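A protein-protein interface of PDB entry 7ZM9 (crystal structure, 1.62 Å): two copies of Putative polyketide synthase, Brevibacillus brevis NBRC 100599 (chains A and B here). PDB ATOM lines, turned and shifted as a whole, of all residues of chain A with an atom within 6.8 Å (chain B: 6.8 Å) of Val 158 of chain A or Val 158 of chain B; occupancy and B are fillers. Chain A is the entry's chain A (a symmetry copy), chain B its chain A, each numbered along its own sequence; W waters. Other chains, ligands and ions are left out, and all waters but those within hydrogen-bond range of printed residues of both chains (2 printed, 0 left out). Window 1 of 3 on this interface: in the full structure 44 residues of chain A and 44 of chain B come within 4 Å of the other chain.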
ATOM      1  N   PHE A 124     -19.351   5.213   6.001  1.00  0.00           N
ATOM      2  CA  PHE A 124     -20.467   5.303   6.934  1.00  0.00           C
ATOM      3  C   PHE A 124     -19.944   5.987   8.189  1.00  0.00           C
ATOM      4  O   PHE A 124     -19.102   5.418   8.879  1.00  0.00           O
ATOM      5  CB  PHE A 124     -21.015   3.906   7.290  1.00  0.00           C
ATOM      6  CG  PHE A 124     -21.470   3.094   6.102  1.00  0.00           C
ATOM      7  CD1 PHE A 124     -20.548   2.427   5.329  1.00  0.00           C
ATOM      8  CD2 PHE A 124     -22.806   3.060   5.734  1.00  0.00           C
ATOM      9  CE1 PHE A 124     -20.999   1.681   4.214  1.00  0.00           C
ATOM     10  CE2 PHE A 124     -23.237   2.355   4.648  1.00  0.00           C
ATOM     11  CZ  PHE A 124     -22.324   1.665   3.882  1.00  0.00           C
ATOM     12  N   VAL A 125     -20.487   7.147   8.537  1.00  0.00           N
ATOM     13  CA  VAL A 125     -19.940   7.913   9.649  1.00  0.00           C
ATOM     14  C   VAL A 125     -21.052   8.429  10.537  1.00  0.00           C
ATOM     15  O   VAL A 125     -22.057   8.962  10.051  1.00  0.00           O
ATOM     16  CB  VAL A 125     -19.040   9.049   9.144  1.00  0.00           C
ATOM     17  CG1 VAL A 125     -19.839  10.060   8.404  1.00  0.00           C
ATOM     18  CG2 VAL A 125     -18.256   9.745  10.332  1.00  0.00           C
ATOM     19  N   GLY A 126     -20.857   8.264  11.850  1.00  0.00           N
ATOM     20  CA  GLY A 126     -21.802   8.725  12.846  1.00  0.00           C
ATOM     21  C   GLY A 126     -21.432  10.080  13.409  1.00  0.00           C
ATOM     22  O   GLY A 126     -20.265  10.346  13.735  1.00  0.00           O
ATOM     23  N   VAL A 127     -22.445  10.952  13.510  1.00  0.00           N
ATOM     24  CA  VAL A 127     -22.243  12.325  13.987  1.00  0.00           C
ATOM     25  C   VAL A 127     -23.570  12.826  14.526  1.00  0.00           C
ATOM     26  O   VAL A 127     -24.635  12.408  14.065  1.00  0.00           O
ATOM     27  CB  VAL A 127     -21.675  13.181  12.839  1.00  0.00           C
ATOM     28  CG1 VAL A 127     -22.654  13.213  11.635  1.00  0.00           C
ATOM     29  CG2 VAL A 127     -21.407  14.643  13.288  1.00  0.00           C
ATOM     30  N   MET A 128     -23.513  13.722  15.531  1.00  0.00           N
ATOM     31  CA  MET A 128     -24.760  14.188  16.099  1.00  0.00           C
ATOM     32  C   MET A 128     -24.809  15.633  16.565  1.00  0.00           C
ATOM     33  O   MET A 128     -25.894  16.107  16.905  1.00  0.00           O
ATOM     34  CB  MET A 128     -25.196  13.309  17.277  1.00  0.00           C
ATOM     35  CG  MET A 128     -24.267  13.492  18.498  1.00  0.00           C
ATOM     36  SD  MET A 128     -24.824  12.569  19.964  1.00  0.00           S
ATOM     37  CE  MET A 128     -26.167  13.514  20.511  1.00  0.00           C
ATOM     38  N   TYR A 138     -23.516  17.493   7.840  1.00  0.00           N
ATOM     39  CA  TYR A 138     -23.022  16.168   8.203  1.00  0.00           C
ATOM     40  C   TYR A 138     -22.645  15.353   6.972  1.00  0.00           C
ATOM     41  O   TYR A 138     -21.636  14.645   6.961  1.00  0.00           O
ATOM     42  CB  TYR A 138     -24.080  15.433   9.005  1.00  0.00           C
ATOM     43  CG  TYR A 138     -24.451  16.014  10.333  1.00  0.00           C
ATOM     44  CD1 TYR A 138     -23.620  16.926  11.016  1.00  0.00           C
ATOM     45  CD2 TYR A 138     -25.619  15.620  10.962  1.00  0.00           C
ATOM     46  CE1 TYR A 138     -24.021  17.452  12.261  1.00  0.00           C
ATOM     47  CE2 TYR A 138     -25.990  16.110  12.213  1.00  0.00           C
ATOM     48  CZ  TYR A 138     -25.202  17.053  12.841  1.00  0.00           C
ATOM     49  OH  TYR A 138     -25.642  17.532  14.069  1.00  0.00           O
ATOM     50  N   VAL A 156     -22.496   8.025   3.550  1.00  0.00           N
ATOM     51  CA  VAL A 156     -23.605   8.510   4.368  1.00  0.00           C
ATOM     52  C   VAL A 156     -23.144   8.930   5.729  1.00  0.00           C
ATOM     53  O   VAL A 156     -22.314   8.249   6.351  1.00  0.00           O
ATOM     54  CB  VAL A 156     -24.717   7.452   4.445  1.00  0.00           C
ATOM     55  CG1 VAL A 156     -24.140   6.143   4.946  1.00  0.00           C
ATOM     56  CG2 VAL A 156     -25.869   7.895   5.278  1.00  0.00           C
ATOM     57  N   ALA A 157     -23.744  10.023   6.218  1.00  0.00           N
ATOM     58  CA  ALA A 157     -23.679  10.417   7.623  1.00  0.00           C
ATOM     59  C   ALA A 157     -24.964   9.991   8.314  1.00  0.00           C
ATOM     60  O   ALA A 157     -26.068  10.208   7.797  1.00  0.00           O
ATOM     61  CB  ALA A 157     -23.483  11.931   7.781  1.00  0.00           C
ATOM     62  N   VAL A 158     -24.827   9.304   9.453  1.00  0.00           N
ATOM     63  CA  VAL A 158     -26.003   8.853  10.183  1.00  0.00           C
ATOM     64  C   VAL A 158     -25.994   9.448  11.586  1.00  0.00           C
ATOM     65  O   VAL A 158     -24.949   9.596  12.243  1.00  0.00           O
ATOM     66  CB  VAL A 158     -26.159   7.323  10.271  1.00  0.00           C
ATOM     67  CG1 VAL A 158     -26.344   6.725   8.859  1.00  0.00           C
ATOM     68  CG2 VAL A 158     -25.011   6.736  10.874  1.00  0.00           C
ATOM     69  N   ASP A 159     -27.185   9.868  11.995  1.00  0.00           N
ATOM     70  CA  ASP A 159     -27.401  10.505  13.297  1.00  0.00           C
ATOM     71  C   ASP A 159     -28.453   9.694  14.037  1.00  0.00           C
ATOM     72  O   ASP A 159     -29.651   9.813  13.773  1.00  0.00           O
ATOM     73  CB  ASP A 159     -27.823  11.966  13.146  1.00  0.00           C
ATOM     74  CG  ASP A 159     -28.034  12.660  14.480  1.00  0.00           C
ATOM     75  OD1 ASP A 159     -27.713  12.035  15.541  1.00  0.00           O
ATOM     76  OD2 ASP A 159     -28.530  13.826  14.462  1.00  0.00           O
ATOM     77  N   THR A 160     -27.996   8.891  14.998  1.00  0.00           N
ATOM     78  CA  THR A 160     -28.856   8.260  15.979  1.00  0.00           C
ATOM     79  C   THR A 160     -28.456   8.736  17.374  1.00  0.00           C
ATOM     80  O   THR A 160     -28.618   8.011  18.366  1.00  0.00           O
ATOM     81  CB  THR A 160     -28.764   6.745  15.908  1.00  0.00           C
ATOM     82  OG1 THR A 160     -27.425   6.279  16.070  1.00  0.00           O
ATOM     83  CG2 THR A 160     -29.223   6.281  14.571  1.00  0.00           C
ATOM     84  N   ALA A 161     -28.031   9.997  17.453  1.00  0.00           N
ATOM     85  CA  ALA A 161     -27.470  10.563  18.694  1.00  0.00           C
ATOM     86  C   ALA A 161     -26.283   9.717  19.142  1.00  0.00           C
ATOM     87  O   ALA A 161     -25.427   9.383  18.324  1.00  0.00           O
ATOM     88  CB  ALA A 161     -28.551  10.666  19.751  1.00  0.00           C
ATOM     89  N   SER A 163     -25.451   6.760  19.811  1.00  0.00           N
ATOM     90  CA  SER A 163     -25.108   5.488  19.265  1.00  0.00           C
ATOM     91  C   SER A 163     -24.598   5.558  17.806  1.00  0.00           C
ATOM     92  O   SER A 163     -24.381   4.525  17.154  1.00  0.00           O
ATOM     93  CB  SER A 163     -26.342   4.563  19.325  1.00  0.00           C
ATOM     94  OG  SER A 163     -27.455   5.192  18.662  1.00  0.00           O
ATOM     95  N   ALA A 164     -24.437   6.785  17.287  1.00  0.00           N
ATOM     96  CA  ALA A 164     -24.300   6.956  15.844  1.00  0.00           C
ATOM     97  C   ALA A 164     -23.135   6.191  15.243  1.00  0.00           C
ATOM     98  O   ALA A 164     -23.292   5.608  14.171  1.00  0.00           O
ATOM     99  CB  ALA A 164     -24.182   8.432  15.508  1.00  0.00           C
ATOM    100  N   SER A 165     -21.949   6.157  15.886  1.00  0.00           N
ATOM    101  CA  SER A 165     -20.857   5.440  15.231  1.00  0.00           C
ATOM    102  C   SER A 165     -21.073   3.933  15.254  1.00  0.00           C
ATOM    103  O   SER A 165     -20.615   3.227  14.341  1.00  0.00           O
ATOM    104  CB  SER A 165     -19.486   5.843  15.804  1.00  0.00           C
ATOM    105  OG  SER A 165     -19.411   5.583  17.186  1.00  0.00           O
ATOM    106  N   THR A 167     -24.145   2.585  15.058  1.00  0.00           N
ATOM    107  CA  THR A 167     -25.109   2.481  13.955  1.00  0.00           C
ATOM    108  C   THR A 167     -24.413   2.464  12.611  1.00  0.00           C
ATOM    109  O   THR A 167     -24.782   1.677  11.720  1.00  0.00           O
ATOM    110  CB  THR A 167     -26.115   3.616  14.059  1.00  0.00           C
ATOM    111  OG1 THR A 167     -26.786   3.505  15.334  1.00  0.00           O
ATOM    112  CG2 THR A 167     -27.118   3.518  12.942  1.00  0.00           C
ATOM    113  N   ALA A 168     -23.462   3.358  12.420  1.00  0.00           N
ATOM    114  CA  ALA A 168     -22.691   3.411  11.199  1.00  0.00           C
ATOM    115  C   ALA A 168     -22.033   2.084  10.885  1.00  0.00           C
ATOM    116  O   ALA A 168     -22.045   1.625   9.730  1.00  0.00           O
ATOM    117  CB  ALA A 168     -21.667   4.517  11.266  1.00  0.00           C
ATOM    118  N   ILE A 169     -21.456   1.427  11.900  1.00  0.00           N
ATOM    119  CA  ILE A 169     -20.888   0.110  11.680  1.00  0.00           C
ATOM    120  C   ILE A 169     -21.960  -0.880  11.248  1.00  0.00           C
ATOM    121  O   ILE A 169     -21.732  -1.713  10.364  1.00  0.00           O
ATOM    122  CB  ILE A 169     -20.129  -0.335  12.963  1.00  0.00           C
ATOM    123  CG1 ILE A 169     -18.897   0.525  13.096  1.00  0.00           C
ATOM    124  CG2 ILE A 169     -19.793  -1.840  12.884  1.00  0.00           C
ATOM    125  CD1 ILE A 169     -18.206   0.408  14.491  1.00  0.00           C
ATOM    126  N   PHE A 171     -24.722  -0.303   9.598  1.00  0.00           N
ATOM    127  CA  PHE A 171     -25.051  -0.081   8.206  1.00  0.00           C
ATOM    128  C   PHE A 171     -23.949  -0.575   7.302  1.00  0.00           C
ATOM    129  O   PHE A 171     -24.234  -1.109   6.202  1.00  0.00           O
ATOM    130  CB  PHE A 171     -25.339   1.401   7.973  1.00  0.00           C
ATOM    131  CG  PHE A 171     -26.718   1.812   8.451  1.00  0.00           C
ATOM    132  CD1 PHE A 171     -27.827   1.188   8.050  1.00  0.00           C
ATOM    133  CD2 PHE A 171     -26.868   2.886   9.292  1.00  0.00           C
ATOM    134  CE1 PHE A 171     -29.078   1.600   8.453  1.00  0.00           C
ATOM    135  CE2 PHE A 171     -28.123   3.294   9.702  1.00  0.00           C
ATOM    136  CZ  PHE A 171     -29.215   2.649   9.279  1.00  0.00           C
ATOM    137  N   GLY A 187     -17.125   4.639  11.012  1.00  0.00           N
ATOM    138  CA  GLY A 187     -16.583   5.305  12.199  1.00  0.00           C
ATOM    139  C   GLY A 187     -17.488   6.407  12.681  1.00  0.00           C
ATOM    140  O   GLY A 187     -18.715   6.376  12.449  1.00  0.00           O
ATOM    141  N   SER A 340     -21.513  10.775  19.646  1.00  0.00           N
ATOM    142  CA  SER A 340     -21.560   9.986  18.432  1.00  0.00           C
ATOM    143  C   SER A 340     -20.314   9.174  18.186  1.00  0.00           C
ATOM    144  O   SER A 340     -20.407   8.165  17.465  1.00  0.00           O
ATOM    145  CB  SER A 340     -21.823  10.920  17.215  1.00  0.00           C
ATOM    146  OG  SER A 340     -21.132  12.183  17.384  1.00  0.00           O
ATOM    147  N   PHE B 124     -37.006   5.667   9.230  1.00  0.00           N
ATOM    148  CA  PHE B 124     -35.849   6.096   8.457  1.00  0.00           C
ATOM    149  C   PHE B 124     -36.205   7.434   7.825  1.00  0.00           C
ATOM    150  O   PHE B 124     -37.090   7.483   6.975  1.00  0.00           O
ATOM    151  CB  PHE B 124     -35.498   5.075   7.356  1.00  0.00           C
ATOM    152  CG  PHE B 124     -35.225   3.680   7.863  1.00  0.00           C
ATOM    153  CD1 PHE B 124     -36.270   2.841   8.171  1.00  0.00           C
ATOM    154  CD2 PHE B 124     -33.927   3.248   8.087  1.00  0.00           C
ATOM    155  CE1 PHE B 124     -35.987   1.542   8.656  1.00  0.00           C
ATOM    156  CE2 PHE B 124     -33.656   2.001   8.571  1.00  0.00           C
ATOM    157  CZ  PHE B 124     -34.696   1.145   8.861  1.00  0.00           C
ATOM    158  N   VAL B 125     -35.480   8.494   8.162  1.00  0.00           N
ATOM    159  CA  VAL B 125     -35.855   9.822   7.696  1.00  0.00           C
ATOM    160  C   VAL B 125     -34.639  10.574   7.198  1.00  0.00           C
ATOM    161  O   VAL B 125     -33.589  10.587   7.853  1.00  0.00           O
ATOM    162  CB  VAL B 125     -36.598  10.599   8.791  1.00  0.00           C
ATOM    163  CG1 VAL B 125     -35.692  10.891   9.933  1.00  0.00           C
ATOM    164  CG2 VAL B 125     -37.214  11.949   8.234  1.00  0.00           C
ATOM    165  N   GLY B 126     -34.796  11.203   6.029  1.00  0.00           N
ATOM    166  CA  GLY B 126     -33.748  11.996   5.420  1.00  0.00           C
ATOM    167  C   GLY B 126     -33.886  13.470   5.729  1.00  0.00           C
ATOM    168  O   GLY B 126     -34.984  14.044   5.662  1.00  0.00           O
ATOM    169  N   VAL B 127     -32.751  14.086   6.087  1.00  0.00           N
ATOM    170  CA  VAL B 127     -32.723  15.503   6.470  1.00  0.00           C
ATOM    171  C   VAL B 127     -31.313  16.015   6.243  1.00  0.00           C
ATOM    172  O   VAL B 127     -30.344  15.258   6.342  1.00  0.00           O
ATOM    173  CB  VAL B 127     -33.210  15.643   7.925  1.00  0.00           C
ATOM    174  CG1 VAL B 127     -32.292  14.850   8.894  1.00  0.00           C
ATOM    175  CG2 VAL B 127     -33.235  17.126   8.385  1.00  0.00           C
ATOM    176  N   MET B 128     -31.189  17.317   5.916  1.00  0.00           N
ATOM    177  CA  MET B 128     -29.862  17.829   5.650  1.00  0.00           C
ATOM    178  C   MET B 128     -29.577  19.261   6.071  1.00  0.00           C
ATOM    179  O   MET B 128     -28.419  19.675   6.004  1.00  0.00           O
ATOM    180  CB  MET B 128     -29.508  17.706   4.163  1.00  0.00           C
ATOM    181  CG  MET B 128     -30.343  18.678   3.298  1.00  0.00           C
ATOM    182  SD  MET B 128     -29.863  18.663   1.542  1.00  0.00           S
ATOM    183  CE  MET B 128     -28.370  19.540   1.557  1.00  0.00           C
ATOM    184  N   TYR B 138     -30.977  16.086  14.391  1.00  0.00           N
ATOM    185  CA  TYR B 138     -31.646  15.283  13.371  1.00  0.00           C
ATOM    186  C   TYR B 138     -32.197  13.985  13.951  1.00  0.00           C
ATOM    187  O   TYR B 138     -33.300  13.552  13.609  1.00  0.00           O
ATOM    188  CB  TYR B 138     -30.674  14.974  12.247  1.00  0.00           C
ATOM    189  CG  TYR B 138     -30.160  16.136  11.457  1.00  0.00           C
ATOM    190  CD1 TYR B 138     -30.814  17.386  11.440  1.00  0.00           C
ATOM    191  CD2 TYR B 138     -29.036  15.993  10.663  1.00  0.00           C
ATOM    192  CE1 TYR B 138     -30.283  18.452  10.687  1.00  0.00           C
ATOM    193  CE2 TYR B 138     -28.540  17.037   9.884  1.00  0.00           C
ATOM    194  CZ  TYR B 138     -29.148  18.275   9.928  1.00  0.00           C
ATOM    195  OH  TYR B 138     -28.586  19.287   9.160  1.00  0.00           O
ATOM    196  N   VAL B 156     -33.593   6.119  12.687  1.00  0.00           N
ATOM    197  CA  VAL B 156     -32.388   6.807  12.231  1.00  0.00           C
ATOM    198  C   VAL B 156     -32.719   7.980  11.362  1.00  0.00           C
ATOM    199  O   VAL B 156     -33.611   7.896  10.504  1.00  0.00           O
ATOM    200  CB  VAL B 156     -31.444   5.822  11.524  1.00  0.00           C
ATOM    201  CG1 VAL B 156     -32.186   5.121  10.403  1.00  0.00           C
ATOM    202  CG2 VAL B 156     -30.202   6.477  11.030  1.00  0.00           C
ATOM    203  N   ALA B 157     -31.941   9.055  11.541  1.00  0.00           N
ATOM    204  CA  ALA B 157     -31.882  10.172  10.601  1.00  0.00           C
ATOM    205  C   ALA B 157     -30.644  10.020   9.733  1.00  0.00           C
ATOM    206  O   ALA B 157     -29.545   9.743  10.231  1.00  0.00           O
ATOM    207  CB  ALA B 157     -31.842  11.524  11.328  1.00  0.00           C
ATOM    208  N   VAL B 158     -30.829  10.118   8.412  1.00  0.00           N
ATOM    209  CA  VAL B 158     -29.702   9.983   7.502  1.00  0.00           C
ATOM    210  C   VAL B 158     -29.557  11.255   6.674  1.00  0.00           C
ATOM    211  O   VAL B 158     -30.537  11.899   6.262  1.00  0.00           O
ATOM    212  CB  VAL B 158     -29.771   8.762   6.565  1.00  0.00           C
ATOM    213  CG1 VAL B 158     -29.742   7.457   7.390  1.00  0.00           C
ATOM    214  CG2 VAL B 158     -30.966   8.792   5.791  1.00  0.00           C
ATOM    215  N   ASP B 159     -28.299  11.649   6.516  1.00  0.00           N
ATOM    216  CA  ASP B 159     -27.931  12.865   5.785  1.00  0.00           C
ATOM    217  C   ASP B 159     -26.979  12.461   4.671  1.00  0.00           C
ATOM    218  O   ASP B 159     -25.791  12.232   4.900  1.00  0.00           O
ATOM    219  CB  ASP B 159     -27.304  13.908   6.709  1.00  0.00           C
ATOM    220  CG  ASP B 159     -26.930  15.189   5.983  1.00  0.00           C
ATOM    221  OD1 ASP B 159     -27.292  15.322   4.771  1.00  0.00           O
ATOM    222  OD2 ASP B 159     -26.268  16.055   6.628  1.00  0.00           O
ATOM    223  N   THR B 160     -27.506  12.412   3.447  1.00  0.00           N
ATOM    224  CA  THR B 160     -26.706  12.319   2.243  1.00  0.00           C
ATOM    225  C   THR B 160     -26.965  13.547   1.373  1.00  0.00           C
ATOM    226  O   THR B 160     -26.868  13.487   0.139  1.00  0.00           O
ATOM    227  CB  THR B 160     -27.026  11.058   1.457  1.00  0.00           C
ATOM    228  OG1 THR B 160     -28.410  10.968   1.125  1.00  0.00           O
ATOM    229  CG2 THR B 160     -26.702   9.863   2.283  1.00  0.00           C
ATOM    230  N   ALA B 161     -27.194  14.683   2.033  1.00  0.00           N
ATOM    231  CA  ALA B 161     -27.607  15.923   1.349  1.00  0.00           C
ATOM    232  C   ALA B 161     -28.884  15.660   0.560  1.00  0.00           C
ATOM    233  O   ALA B 161     -29.817  15.058   1.088  1.00  0.00           O
ATOM    234  CB  ALA B 161     -26.475  16.437   0.482  1.00  0.00           C
ATOM    235  N   SER B 163     -30.116  13.749  -1.611  1.00  0.00           N
ATOM    236  CA  SER B 163     -30.670  12.457  -1.855  1.00  0.00           C
ATOM    237  C   SER B 163     -31.230  11.773  -0.585  1.00  0.00           C
ATOM    238  O   SER B 163     -31.628  10.599  -0.614  1.00  0.00           O
ATOM    239  CB  SER B 163     -29.586  11.553  -2.480  1.00  0.00           C
ATOM    240  OG  SER B 163     -28.423  11.529  -1.630  1.00  0.00           O
ATOM    241  N   ALA B 164     -31.231  12.507   0.538  1.00  0.00           N
ATOM    242  CA  ALA B 164     -31.406  11.859   1.834  1.00  0.00           C
ATOM    243  C   ALA B 164     -32.698  11.073   1.957  1.00  0.00           C
ATOM    244  O   ALA B 164     -32.680   9.974   2.510  1.00  0.00           O
ATOM    245  CB  ALA B 164     -31.318  12.892   2.944  1.00  0.00           C
ATOM    246  N   SER B 165     -33.845  11.582   1.459  1.00  0.00           N
ATOM    247  CA  SER B 165     -35.061  10.793   1.651  1.00  0.00           C
ATOM    248  C   SER B 165     -35.071   9.546   0.778  1.00  0.00           C
ATOM    249  O   SER B 165     -35.671   8.527   1.160  1.00  0.00           O
ATOM    250  CB  SER B 165     -36.329  11.648   1.465  1.00  0.00           C
ATOM    251  OG  SER B 165     -36.379  12.220   0.180  1.00  0.00           O
ATOM    252  N   THR B 167     -32.247   7.879   0.045  1.00  0.00           N
ATOM    253  CA  THR B 167     -31.361   7.034   0.855  1.00  0.00           C
ATOM    254  C   THR B 167     -32.113   6.371   1.989  1.00  0.00           C
ATOM    255  O   THR B 167     -31.907   5.176   2.269  1.00  0.00           O
ATOM    256  CB  THR B 167     -30.193   7.867   1.357  1.00  0.00           C
ATOM    257  OG1 THR B 167     -29.489   8.390   0.210  1.00  0.00           O
ATOM    258  CG2 THR B 167     -29.268   7.012   2.182  1.00  0.00           C
ATOM    259  N   ALA B 168     -32.928   7.135   2.692  1.00  0.00           N
ATOM    260  CA  ALA B 168     -33.738   6.609   3.767  1.00  0.00           C
ATOM    261  C   ALA B 168     -34.600   5.450   3.314  1.00  0.00           C
ATOM    262  O   ALA B 168     -34.709   4.428   4.013  1.00  0.00           O
ATOM    263  CB  ALA B 168     -34.580   7.702   4.377  1.00  0.00           C
ATOM    264  N   ILE B 169     -35.221   5.569   2.133  1.00  0.00           N
ATOM    265  CA  ILE B 169     -35.989   4.457   1.605  1.00  0.00           C
ATOM    266  C   ILE B 169     -35.097   3.248   1.358  1.00  0.00           C
ATOM    267  O   ILE B 169     -35.487   2.108   1.634  1.00  0.00           O
ATOM    268  CB  ILE B 169     -36.745   4.925   0.328  1.00  0.00           C
ATOM    269  CG1 ILE B 169     -37.828   5.884   0.757  1.00  0.00           C
ATOM    270  CG2 ILE B 169     -37.305   3.705  -0.433  1.00  0.00           C
ATOM    271  CD1 ILE B 169     -38.464   6.672  -0.431  1.00  0.00           C
ATOM    272  N   PHE B 171     -32.358   2.383   2.919  1.00  0.00           N
ATOM    273  CA  PHE B 171     -32.065   1.736   4.181  1.00  0.00           C
ATOM    274  C   PHE B 171     -33.268   0.992   4.702  1.00  0.00           C
ATOM    275  O   PHE B 171     -33.117  -0.101   5.301  1.00  0.00           O
ATOM    276  CB  PHE B 171     -31.570   2.771   5.190  1.00  0.00           C
ATOM    277  CG  PHE B 171     -30.124   3.168   4.960  1.00  0.00           C
ATOM    278  CD1 PHE B 171     -29.141   2.270   4.892  1.00  0.00           C
ATOM    279  CD2 PHE B 171     -29.777   4.491   4.859  1.00  0.00           C
ATOM    280  CE1 PHE B 171     -27.825   2.645   4.732  1.00  0.00           C
ATOM    281  CE2 PHE B 171     -28.458   4.867   4.690  1.00  0.00           C
ATOM    282  CZ  PHE B 171     -27.495   3.941   4.630  1.00  0.00           C
ATOM    283  N   GLY B 187     -39.060   8.336   4.865  1.00  0.00           N
ATOM    284  CA  GLY B 187     -39.442   9.623   4.280  1.00  0.00           C
ATOM    285  C   GLY B 187     -38.362  10.657   4.456  1.00  0.00           C
ATOM    286  O   GLY B 187     -37.165  10.319   4.575  1.00  0.00           O
ATOM    287  N   SER B 340     -33.415  17.516   0.953  1.00  0.00           N
ATOM    288  CA  SER B 340     -33.542  16.186   1.515  1.00  0.00           C
ATOM    289  C   SER B 340     -34.905  15.572   1.321  1.00  0.00           C
ATOM    290  O   SER B 340     -34.997  14.333   1.348  1.00  0.00           O
ATOM    291  CB  SER B 340     -33.199  16.227   3.032  1.00  0.00           C
ATOM    292  OG  SER B 340     -33.686  17.455   3.631  1.00  0.00           O
HETATM  293  O   HOH W   1     -28.003  16.388  14.912  1.00  0.00           O
HETATM  294  O   HOH W   2     -26.385  18.474   7.714  1.00  0.00           O
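The backbone NH of Asp 159 of chain B lies within hydrogen-bond range of the backbone carbonyl oxygen of Ala 157 of chain A, 2.9 Å away.
The side-chain carboxylate (OD2) of Asp 159 of chain B lies close to the backbone NH (N) of Tyr 138 of chain A, at 3.3 Å.
N of Tyr 138 of chain B lies close to OD2 of Asp 159 of chain A.
O of Ala 157 of chain B sits at hydrogen-bond distance from N of Asp 159 of chain A.
OG1 of Thr 167 of chain B is in hydrogen-bond range of OG1 of Thr 160 of chain B (2.9 Å).
OG1 of Thr 160 of chain B lies close to N of Ala 164 of chain B.
O of Met 128 of chain A is in hydrogen-bond range of OH of Tyr 138 of chain A (3.2 Å).
OG of Ser 163 of chain A sits at hydrogen-bond distance from OG1 of Thr 160 of chain A.
OD1 of Asp 159 of chain B lies within hydrogen-bond range of N of Ala 161 of chain B (2.8 Å).
The side-chain hydroxyl (OG1) of Thr 160 of chain B sits at hydrogen-bond distance from the side-chain hydroxyl (OG) of Ser 163 of chain B (2.8 Å).
Tyr 138 of chain B touches Tyr 138 of chain A (CD2 to CE2, 3.4 Å).
Val 156 of chain A touches Thr 160 of chain B.
O of Ala 157 of chain A touches CA of Val 158 of chain B, at 3.7 Å.
CA of Val 158 of chain A touches O of Ala 157 of chain B (3.7 Å).
Val 158 of chain A touches Val 158 of chain B.
Thr 160 of chain A touches Val 156 of chain B (CG2 to CG2, 3.7 Å).
CD1 of Phe 171 of chain B touches CD1 of Phe 171 of chain A (3.6 Å).
Printed residues of chain B within 4 Å of Tyr 138 of chain A: Tyr 138 (3.4 Å) and Asp 159 (3.3 Å).
Of the printed residues of chain B, Val 156 of chain A touches Thr 160.
Printed residues of chain B within 4 Å of Val 158 of chain A: Ala 157 (3.7 Å) and Val 158 (3.8 Å).
Of the printed residues of chain B, Asp 159 of chain A touches Tyr 138 and Ala 157.
Val 125 of chain B touches none of the printed residues of chain A.
Of the printed residues of chain A, Ala 157 of chain B touches Val 158 (3.7 Å) and Asp 159 (2.9 Å).
Printed residues of chain A within 4 Å of Val 158 of chain B: Ala 157 and Val 158.
Among the printed residues, no Asp or Glu carboxylate lies within 4 Å of a Lys or Arg side-chain nitrogen of the other chain.
Val 156 of chain A touches Thr 160 of chain B, and with the chains exchanged Thr 160 of chain A touches Val 156 of chain B.
Ala 157 of chain A touches Val 158 of chain B, and with the chains exchanged Val 158 of chain A touches Ala 157 of chain B.
Ala 157 of chain A touches Asp 159 of chain B, and with the chains exchanged Asp 159 of chain A touches Ala 157 of chain B.
Phe 171 of chain B touches its own counterpart, Phe 171 of chain A.
Water W1 lies within hydrogen-bond range of OD2 of Asp 159 of chain A (2.7 Å), OH of Tyr 138 of chain A (2.8 Å), O of Met 128 of chain A (2.9 Å) and N of Tyr 138 of chain B (3.0 Å).
Water W2 lies within hydrogen-bond range of the side-chain carboxylate (OD2) of Asp 159 of chain B (2.7 Å), the side-chain hydroxyl (OH) of Tyr 138 of chain B (2.8 Å), the backbone carbonyl oxygen (O) of Met 128 of chain B (2.9 Å) and the backbone NH (N) of Tyr 138 of chain A (3.0 Å).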
